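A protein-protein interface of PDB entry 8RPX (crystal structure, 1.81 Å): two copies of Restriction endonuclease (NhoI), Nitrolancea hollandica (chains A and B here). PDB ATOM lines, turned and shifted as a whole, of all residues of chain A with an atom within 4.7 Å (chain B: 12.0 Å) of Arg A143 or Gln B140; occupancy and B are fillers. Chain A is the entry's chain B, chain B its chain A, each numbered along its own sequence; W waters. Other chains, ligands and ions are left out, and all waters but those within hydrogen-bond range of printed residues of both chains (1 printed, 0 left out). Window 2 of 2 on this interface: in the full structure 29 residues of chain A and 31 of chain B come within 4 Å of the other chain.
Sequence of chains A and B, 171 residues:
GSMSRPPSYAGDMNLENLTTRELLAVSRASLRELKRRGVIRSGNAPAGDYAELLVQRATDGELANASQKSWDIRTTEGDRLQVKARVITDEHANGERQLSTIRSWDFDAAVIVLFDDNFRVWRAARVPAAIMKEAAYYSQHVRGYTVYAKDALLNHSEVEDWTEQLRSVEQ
Water W1 bridges a ring nitrogen (ND1) of His A141 (2.5 Å) and the guanidinium group (NH2) of Arg B143 (3.3 Å).
The guanidinium group (NE) of Arg B143 sits at hydrogen-bond distance from the backbone carbonyl oxygen (O) of His A141, at 2.9 Å. The backbone carbonyl oxygen of His B141 sits at hydrogen-bond distance from the guanidinium group of Arg A143, at 2.9 Å. NE of Arg B143 is in hydrogen-bond range of O of Gln A140, at 3.4 Å. The guanidinium group (NH2) of Arg A103 sits close to the guanidinium group (NH2) of Arg B103 (3.4 Å). The guanidinium group of Arg B103 lies within hydrogen-bond range of the backbone carbonyl oxygen of His A141, at 3.3 Å. O of Gln B140 lies within hydrogen-bond range of NE of Arg A143. The backbone carbonyl oxygen (O) of His B141 lies within hydrogen-bond range of the guanidinium group (NE) of Arg A103.
Hydrophobic or aromatic side chains of chain B within 4 Å of the printed part of chain A: His B141 and Val B142. Of the 8 printed residues of chain A, 5 touch a printed residue of chain B. Along chain A the printed residues that touch a printed residue of chain B span positions 103 to 143. Among the printed residues, no Asp or Glu carboxylate lies within 4 Å of a Lys or Arg side-chain nitrogen of the other chain.
Among the printed residues, merely in contact across the chains: Arg A103 with Val B142 (3.9 Å), Val A142 with Arg B103 (3.9 Å) and Val A142 with Val B142 (3.9 Å).
Arg B103 touches its own counterpart, Arg A103. Arg A103 touches His B141, and with the chains exchanged His A141 touches Arg B103. His A141 touches Arg B143, and with the chains exchanged Arg A143 touches His B141. Val B142 touches its own counterpart, Val A142. Positions printed for both chains: 103, 138, 139, 140, 141, 142, 143 and 144. Of the 10 pairs that touch across the chains among the printed residues, 10 have their exchanged pair printed and touching as well.
Arg A143 touches just these residues of chain B: Gln B140 and His B141. Printed residues of chain A within 4 Å of Gln B140: Arg A143. Of chain B, only Arg B103 (3.4 Å), His B141 (3.3 Å) and Val B142 (3.9 Å) come within 4 Å of Arg A103. No residue of chain B comes within 4 Å of Ser A139. Val A142 touches two residues of chain B. Gly A144 touches none of the printed residues of chain B. Printed residues of chain A within 4 Å of His B141: Arg A103 and Arg A143. Printed residues of chain A within 4 Å of Val B142: Arg A103 (3.9 Å) and Val A142 (3.9 Å). Of the printed residues of chain A, Arg B143 touches Gln A140 (3.4 Å) and His A141 (2.9 Å). Of the printed residues of chain B, Gln A140 touches Arg B143. Tyr B137 touches none of the printed residues of chain A. The nearest printed residue of chain A that does not touch Gln B140 is Val A142 (6.5 Å).
The backbone carbonyl oxygen of Arg A143 sits close to the guanidinium group of Arg A103 (3.4 Å). The backbone carbonyl oxygen (O) of Arg B143 lies close to the guanidinium group (NE) of Arg B103 (3.4 Å). NH2 of Arg A103 is in hydrogen-bond range of O of Val A142 (2.8 Å). The backbone carbonyl oxygen of Val B142 sits at hydrogen-bond distance from the guanidinium group of Arg B103 (2.8 Å).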
ATOM      1  N   ARG A 103      -2.246  22.187 -17.150  1.00  0.00           N
ATOM      2  CA  ARG A 103      -2.764  20.874 -16.787  1.00  0.00           C
ATOM      3  C   ARG A 103      -1.892  20.163 -15.775  1.00  0.00           C
ATOM      4  O   ARG A 103      -2.249  19.070 -15.329  1.00  0.00           O
ATOM      5  CB  ARG A 103      -2.948  20.000 -18.036  1.00  0.00           C
ATOM      6  CG  ARG A 103      -4.022  20.556 -18.979  1.00  0.00           C
ATOM      7  CD  ARG A 103      -4.345  19.608 -20.142  1.00  0.00           C
ATOM      8  NE  ARG A 103      -5.533  20.047 -20.868  1.00  0.00           N
ATOM      9  CZ  ARG A 103      -5.511  20.702 -22.019  1.00  0.00           C
ATOM     10  NH1 ARG A 103      -4.371  21.032 -22.608  1.00  0.00           N
ATOM     11  NH2 ARG A 103      -6.662  21.063 -22.584  1.00  0.00           N
ATOM     12  N   TYR A 138     -10.549  26.409 -12.564  1.00  0.00           N
ATOM     13  CA  TYR A 138     -10.563  25.169 -13.317  1.00  0.00           C
ATOM     14  C   TYR A 138     -11.599  25.253 -14.422  1.00  0.00           C
ATOM     15  O   TYR A 138     -12.658  25.871 -14.259  1.00  0.00           O
ATOM     16  CB  TYR A 138     -10.849  23.986 -12.396  1.00  0.00           C
ATOM     17  CG  TYR A 138     -10.790  22.653 -13.105  1.00  0.00           C
ATOM     18  CD1 TYR A 138      -9.575  22.133 -13.551  1.00  0.00           C
ATOM     19  CD2 TYR A 138     -11.934  21.879 -13.253  1.00  0.00           C
ATOM     20  CE1 TYR A 138      -9.519  20.890 -14.188  1.00  0.00           C
ATOM     21  CE2 TYR A 138     -11.888  20.646 -13.871  1.00  0.00           C
ATOM     22  CZ  TYR A 138     -10.680  20.159 -14.337  1.00  0.00           C
ATOM     23  OH  TYR A 138     -10.661  18.932 -14.951  1.00  0.00           O
ATOM     24  N   SER A 139     -11.271  24.664 -15.565  1.00  0.00           N
ATOM     25  CA  SER A 139     -12.193  24.574 -16.686  1.00  0.00           C
ATOM     26  C   SER A 139     -12.416  23.092 -16.978  1.00  0.00           C
ATOM     27  O   SER A 139     -11.497  22.399 -17.432  1.00  0.00           O
ATOM     28  CB  SER A 139     -11.645  25.309 -17.908  1.00  0.00           C
ATOM     29  OG  SER A 139     -12.451  25.029 -19.039  1.00  0.00           O
ATOM     30  N   GLN A 140     -13.623  22.597 -16.686  1.00  0.00           N
ATOM     31  CA  GLN A 140     -13.899  21.191 -16.948  1.00  0.00           C
ATOM     32  C   GLN A 140     -13.927  20.893 -18.445  1.00  0.00           C
ATOM     33  O   GLN A 140     -13.650  19.761 -18.856  1.00  0.00           O
ATOM     34  CB  GLN A 140     -15.216  20.792 -16.298  1.00  0.00           C
ATOM     35  CG  GLN A 140     -15.511  19.319 -16.397  1.00  0.00           C
ATOM     36  CD  GLN A 140     -16.849  19.045 -17.047  1.00  0.00           C
ATOM     37  OE1 GLN A 140     -17.898  19.231 -16.424  1.00  0.00           O
ATOM     38  NE2 GLN A 140     -16.826  18.612 -18.310  1.00  0.00           N
ATOM     39  N   HIS A 141     -14.243  21.894 -19.268  1.00  0.00           N
ATOM     40  CA  HIS A 141     -14.332  21.689 -20.711  1.00  0.00           C
ATOM     41  C   HIS A 141     -12.998  21.242 -21.314  1.00  0.00           C
ATOM     42  O   HIS A 141     -12.966  20.403 -22.228  1.00  0.00           O
ATOM     43  CB  HIS A 141     -14.823  22.973 -21.376  1.00  0.00           C
ATOM     44  CG  HIS A 141     -14.932  22.881 -22.868  1.00  0.00           C
ATOM     45  ND1 HIS A 141     -15.787  22.007 -23.501  1.00  0.00           N
ATOM     46  CD2 HIS A 141     -14.291  23.560 -23.852  1.00  0.00           C
ATOM     47  CE1 HIS A 141     -15.666  22.142 -24.811  1.00  0.00           C
ATOM     48  NE2 HIS A 141     -14.767  23.082 -25.051  1.00  0.00           N
ATOM     49  N   VAL A 142     -11.889  21.791 -20.826  1.00  0.00           N
ATOM     50  CA  VAL A 142     -10.565  21.486 -21.359  1.00  0.00           C
ATOM     51  C   VAL A 142      -9.721  20.685 -20.390  1.00  0.00           C
ATOM     52  O   VAL A 142      -8.564  20.352 -20.721  1.00  0.00           O
ATOM     53  CB  VAL A 142      -9.817  22.767 -21.768  1.00  0.00           C
ATOM     54  CG1 VAL A 142     -10.642  23.555 -22.783  1.00  0.00           C
ATOM     55  CG2 VAL A 142      -9.475  23.609 -20.518  1.00  0.00           C
ATOM     56  N   ARG A 143     -10.250  20.372 -19.205  1.00  0.00           N
ATOM     57  CA  ARG A 143      -9.529  19.641 -18.156  1.00  0.00           C
ATOM     58  C   ARG A 143      -8.216  20.357 -17.824  1.00  0.00           C
ATOM     59  O   ARG A 143      -7.128  19.792 -17.879  1.00  0.00           O
ATOM     60  CB  ARG A 143      -9.297  18.165 -18.562  1.00  0.00           C
ATOM     61  CG  ARG A 143      -9.045  17.208 -17.391  1.00  0.00           C
ATOM     62  CD  ARG A 143      -8.503  15.828 -17.834  1.00  0.00           C
ATOM     63  NE  ARG A 143      -7.129  15.973 -18.303  1.00  0.00           N
ATOM     64  CZ  ARG A 143      -6.087  16.157 -17.507  1.00  0.00           C
ATOM     65  NH1 ARG A 143      -6.201  16.062 -16.190  1.00  0.00           N
ATOM     66  NH2 ARG A 143      -4.910  16.470 -18.039  1.00  0.00           N
ATOM     67  N   GLY A 144      -8.341  21.636 -17.457  1.00  0.00           N
ATOM     68  CA  GLY A 144      -7.148  22.418 -17.192  1.00  0.00           C
ATOM     69  C   GLY A 144      -7.502  23.679 -16.430  1.00  0.00           C
ATOM     70  O   GLY A 144      -8.674  24.020 -16.272  1.00  0.00           O
ATOM     71  N   GLN B  98      -2.781  15.677 -38.294  1.00  0.00           N
ATOM     72  CA  GLN B  98      -3.552  15.663 -37.059  1.00  0.00           C
ATOM     73  C   GLN B  98      -4.405  16.918 -36.976  1.00  0.00           C
ATOM     74  O   GLN B  98      -3.877  18.034 -36.960  1.00  0.00           O
ATOM     75  CB  GLN B  98      -2.642  15.580 -35.843  1.00  0.00           C
ATOM     76  CG  GLN B  98      -3.421  15.543 -34.539  1.00  0.00           C
ATOM     77  CD  GLN B  98      -2.512  15.410 -33.359  1.00  0.00           C
ATOM     78  OE1 GLN B  98      -1.442  14.817 -33.469  1.00  0.00           O
ATOM     79  NE2 GLN B  98      -2.931  15.935 -32.220  1.00  0.00           N
ATOM     80  N   THR B 101      -8.402  19.299 -31.911  1.00  0.00           N
ATOM     81  CA  THR B 101      -9.205  18.370 -31.134  1.00  0.00           C
ATOM     82  C   THR B 101     -10.699  18.653 -31.290  1.00  0.00           C
ATOM     83  O   THR B 101     -11.132  19.791 -31.487  1.00  0.00           O
ATOM     84  CB  THR B 101      -8.798  18.435 -29.651  1.00  0.00           C
ATOM     85  OG1 THR B 101      -9.285  17.271 -28.971  1.00  0.00           O
ATOM     86  CG2 THR B 101      -9.378  19.675 -28.979  1.00  0.00           C
ATOM     87  N   ILE B 102     -11.498  17.597 -31.194  1.00  0.00           N
ATOM     88  CA  ILE B 102     -12.947  17.689 -31.328  1.00  0.00           C
ATOM     89  C   ILE B 102     -13.533  17.306 -29.981  1.00  0.00           C
ATOM     90  O   ILE B 102     -13.313  16.189 -29.500  1.00  0.00           O
ATOM     91  CB  ILE B 102     -13.492  16.775 -32.446  1.00  0.00           C
ATOM     92  CG1 ILE B 102     -13.077  17.260 -33.848  1.00  0.00           C
ATOM     93  CG2 ILE B 102     -14.999  16.665 -32.349  1.00  0.00           C
ATOM     94  CD1 ILE B 102     -13.369  16.217 -34.965  1.00  0.00           C
ATOM     95  N   ARG B 103     -14.281  18.220 -29.371  1.00  0.00           N
ATOM     96  CA  ARG B 103     -14.899  17.959 -28.079  1.00  0.00           C
ATOM     97  C   ARG B 103     -16.404  17.840 -28.178  1.00  0.00           C
ATOM     98  O   ARG B 103     -17.063  17.504 -27.186  1.00  0.00           O
ATOM     99  CB  ARG B 103     -14.526  19.073 -27.085  1.00  0.00           C
ATOM    100  CG  ARG B 103     -13.052  19.108 -26.757  1.00  0.00           C
ATOM    101  CD  ARG B 103     -12.753  20.101 -25.635  1.00  0.00           C
ATOM    102  NE  ARG B 103     -11.401  19.933 -25.115  1.00  0.00           N
ATOM    103  CZ  ARG B 103     -10.372  20.706 -25.426  1.00  0.00           C
ATOM    104  NH1 ARG B 103     -10.493  21.703 -26.288  1.00  0.00           N
ATOM    105  NH2 ARG B 103      -9.197  20.484 -24.842  1.00  0.00           N
ATOM    106  N   ALA B 136     -11.880   8.600 -35.128  1.00  0.00           N
ATOM    107  CA  ALA B 136     -11.381   9.386 -34.010  1.00  0.00           C
ATOM    108  C   ALA B 136     -10.865   8.495 -32.889  1.00  0.00           C
ATOM    109  O   ALA B 136     -11.371   7.392 -32.658  1.00  0.00           O
ATOM    110  CB  ALA B 136     -12.481  10.294 -33.467  1.00  0.00           C
ATOM    111  N   TYR B 137      -9.844   8.988 -32.187  1.00  0.00           N
ATOM    112  CA  TYR B 137      -9.312   8.379 -30.973  1.00  0.00           C
ATOM    113  C   TYR B 137      -9.450   9.380 -29.831  1.00  0.00           C
ATOM    114  O   TYR B 137      -9.190  10.564 -30.033  1.00  0.00           O
ATOM    115  CB  TYR B 137      -7.832   8.000 -31.135  1.00  0.00           C
ATOM    116  CG  TYR B 137      -7.456   7.328 -32.446  1.00  0.00           C
ATOM    117  CD1 TYR B 137      -7.072   8.081 -33.552  1.00  0.00           C
ATOM    118  CD2 TYR B 137      -7.452   5.943 -32.564  1.00  0.00           C
ATOM    119  CE1 TYR B 137      -6.711   7.469 -34.742  1.00  0.00           C
ATOM    120  CE2 TYR B 137      -7.095   5.323 -33.749  1.00  0.00           C
ATOM    121  CZ  TYR B 137      -6.727   6.091 -34.832  1.00  0.00           C
ATOM    122  OH  TYR B 137      -6.369   5.485 -36.006  1.00  0.00           O
ATOM    123  N   TYR B 138      -9.831   8.911 -28.650  1.00  0.00           N
ATOM    124  CA  TYR B 138     -10.085   9.808 -27.532  1.00  0.00           C
ATOM    125  C   TYR B 138      -8.791  10.090 -26.785  1.00  0.00           C
ATOM    126  O   TYR B 138      -7.948   9.202 -26.610  1.00  0.00           O
ATOM    127  CB  TYR B 138     -11.130   9.208 -26.586  1.00  0.00           C
ATOM    128  CG  TYR B 138     -11.534  10.132 -25.455  1.00  0.00           C
ATOM    129  CD1 TYR B 138     -12.306  11.254 -25.704  1.00  0.00           C
ATOM    130  CD2 TYR B 138     -11.185   9.856 -24.135  1.00  0.00           C
ATOM    131  CE1 TYR B 138     -12.692  12.105 -24.681  1.00  0.00           C
ATOM    132  CE2 TYR B 138     -11.568  10.706 -23.103  1.00  0.00           C
ATOM    133  CZ  TYR B 138     -12.323  11.831 -23.391  1.00  0.00           C
ATOM    134  OH  TYR B 138     -12.717  12.688 -22.382  1.00  0.00           O
ATOM    135  N   SER B 139      -8.642  11.342 -26.351  1.00  0.00           N
ATOM    136  CA  SER B 139      -7.510  11.787 -25.548  1.00  0.00           C
ATOM    137  C   SER B 139      -8.044  12.287 -24.213  1.00  0.00           C
ATOM    138  O   SER B 139      -8.604  13.388 -24.141  1.00  0.00           O
ATOM    139  CB  SER B 139      -6.738  12.895 -26.259  1.00  0.00           C
ATOM    140  OG  SER B 139      -5.808  13.478 -25.365  1.00  0.00           O
ATOM    141  N   GLN B 140      -7.823  11.504 -23.154  1.00  0.00           N
ATOM    142  CA  GLN B 140      -8.302  11.895 -21.837  1.00  0.00           C
ATOM    143  C   GLN B 140      -7.568  13.127 -21.317  1.00  0.00           C
ATOM    144  O   GLN B 140      -8.124  13.865 -20.502  1.00  0.00           O
ATOM    145  CB  GLN B 140      -8.165  10.728 -20.858  1.00  0.00           C
ATOM    146  CG  GLN B 140      -6.742  10.212 -20.715  1.00  0.00           C
ATOM    147  CD  GLN B 140      -6.659   8.901 -19.945  1.00  0.00           C
ATOM    148  OE1 GLN B 140      -7.654   8.417 -19.398  1.00  0.00           O
ATOM    149  NE2 GLN B 140      -5.466   8.316 -19.904  1.00  0.00           N
ATOM    150  N   HIS B 141      -6.336  13.362 -21.786  1.00  0.00           N
ATOM    151  CA  HIS B 141      -5.532  14.498 -21.331  1.00  0.00           C
ATOM    152  C   HIS B 141      -6.210  15.834 -21.639  1.00  0.00           C
ATOM    153  O   HIS B 141      -6.092  16.794 -20.863  1.00  0.00           O
ATOM    154  CB  HIS B 141      -4.146  14.433 -21.990  1.00  0.00           C
ATOM    155  CG  HIS B 141      -3.222  15.557 -21.613  1.00  0.00           C
ATOM    156  ND1 HIS B 141      -2.799  15.774 -20.318  1.00  0.00           N
ATOM    157  CD2 HIS B 141      -2.607  16.499 -22.369  1.00  0.00           C
ATOM    158  CE1 HIS B 141      -1.984  16.815 -20.289  1.00  0.00           C
ATOM    159  NE2 HIS B 141      -1.843  17.269 -21.521  1.00  0.00           N
ATOM    160  N   VAL B 142      -6.879  15.929 -22.784  1.00  0.00           N
ATOM    161  CA  VAL B 142      -7.510  17.168 -23.229  1.00  0.00           C
ATOM    162  C   VAL B 142      -9.027  17.072 -23.261  1.00  0.00           C
ATOM    163  O   VAL B 142      -9.689  18.065 -23.609  1.00  0.00           O
ATOM    164  CB  VAL B 142      -6.967  17.626 -24.598  1.00  0.00           C
ATOM    165  CG1 VAL B 142      -5.448  17.779 -24.549  1.00  0.00           C
ATOM    166  CG2 VAL B 142      -7.428  16.677 -25.764  1.00  0.00           C
ATOM    167  N   ARG B 143      -9.598  15.919 -22.900  1.00  0.00           N
ATOM    168  CA  ARG B 143     -11.043  15.681 -22.966  1.00  0.00           C
ATOM    169  C   ARG B 143     -11.564  15.980 -24.374  1.00  0.00           C
ATOM    170  O   ARG B 143     -12.481  16.777 -24.574  1.00  0.00           O
ATOM    171  CB  ARG B 143     -11.800  16.491 -21.907  1.00  0.00           C
ATOM    172  CG  ARG B 143     -13.095  15.819 -21.420  1.00  0.00           C
ATOM    173  CD  ARG B 143     -14.017  16.809 -20.696  1.00  0.00           C
ATOM    174  NE  ARG B 143     -14.371  17.901 -21.595  1.00  0.00           N
ATOM    175  CZ  ARG B 143     -15.400  17.882 -22.431  1.00  0.00           C
ATOM    176  NH1 ARG B 143     -16.274  16.883 -22.429  1.00  0.00           N
ATOM    177  NH2 ARG B 143     -15.551  18.884 -23.298  1.00  0.00           N
ATOM    178  N   GLY B 144     -10.957  15.329 -25.363  1.00  0.00           N
ATOM    179  CA  GLY B 144     -11.375  15.551 -26.733  1.00  0.00           C
ATOM    180  C   GLY B 144     -10.962  14.411 -27.640  1.00  0.00           C
ATOM    181  O   GLY B 144     -10.214  13.512 -27.251  1.00  0.00           O
ATOM    182  N   TYR B 145     -11.457  14.473 -28.873  1.00  0.00           N
ATOM    183  CA  TYR B 145     -11.222  13.453 -29.881  1.00  0.00           C
ATOM    184  C   TYR B 145     -10.280  13.958 -30.964  1.00  0.00           C
ATOM    185  O   TYR B 145     -10.447  15.072 -31.478  1.00  0.00           O
ATOM    186  CB  TYR B 145     -12.532  13.021 -30.524  1.00  0.00           C
ATOM    187  CG  TYR B 145     -13.434  12.250 -29.599  1.00  0.00           C
ATOM    188  CD1 TYR B 145     -14.305  12.912 -28.742  1.00  0.00           C
ATOM    189  CD2 TYR B 145     -13.417  10.866 -29.580  1.00  0.00           C
ATOM    190  CE1 TYR B 145     -15.137  12.214 -27.894  1.00  0.00           C
ATOM    191  CE2 TYR B 145     -14.248  10.158 -28.728  1.00  0.00           C
ATOM    192  CZ  TYR B 145     -15.107  10.841 -27.895  1.00  0.00           C
ATOM    193  OH  TYR B 145     -15.938  10.148 -27.049  1.00  0.00           O
ATOM    194  N   THR B 146      -9.343  13.094 -31.352  1.00  0.00           N
ATOM    195  CA  THR B 146      -8.339  13.374 -32.373  1.00  0.00           C
ATOM    196  C   THR B 146      -8.661  12.586 -33.634  1.00  0.00           C
ATOM    197  O   THR B 146      -8.789  11.353 -33.581  1.00  0.00           O
ATOM    198  CB  THR B 146      -6.938  12.977 -31.897  1.00  0.00           C
ATOM    199  OG1 THR B 146      -6.617  13.659 -30.676  1.00  0.00           O
ATOM    200  CG2 THR B 146      -5.897  13.306 -32.961  1.00  0.00           C
ATOM    201  N   VAL B 147      -8.754  13.300 -34.764  1.00  0.00           N
ATOM    202  CA  VAL B 147      -8.930  12.711 -36.088  1.00  0.00           C
ATOM    203  C   VAL B 147      -7.751  13.130 -36.955  1.00  0.00           C
ATOM    204  O   VAL B 147      -7.312  14.285 -36.894  1.00  0.00           O
ATOM    205  CB  VAL B 147     -10.256  13.146 -36.738  1.00  0.00           C
ATOM    206  CG1 VAL B 147     -10.341  12.629 -38.189  1.00  0.00           C
ATOM    207  CG2 VAL B 147     -11.429  12.649 -35.905  1.00  0.00           C
HETATM  208  O   HOH W   1     -17.801  21.062 -22.281  1.00  0.00           O
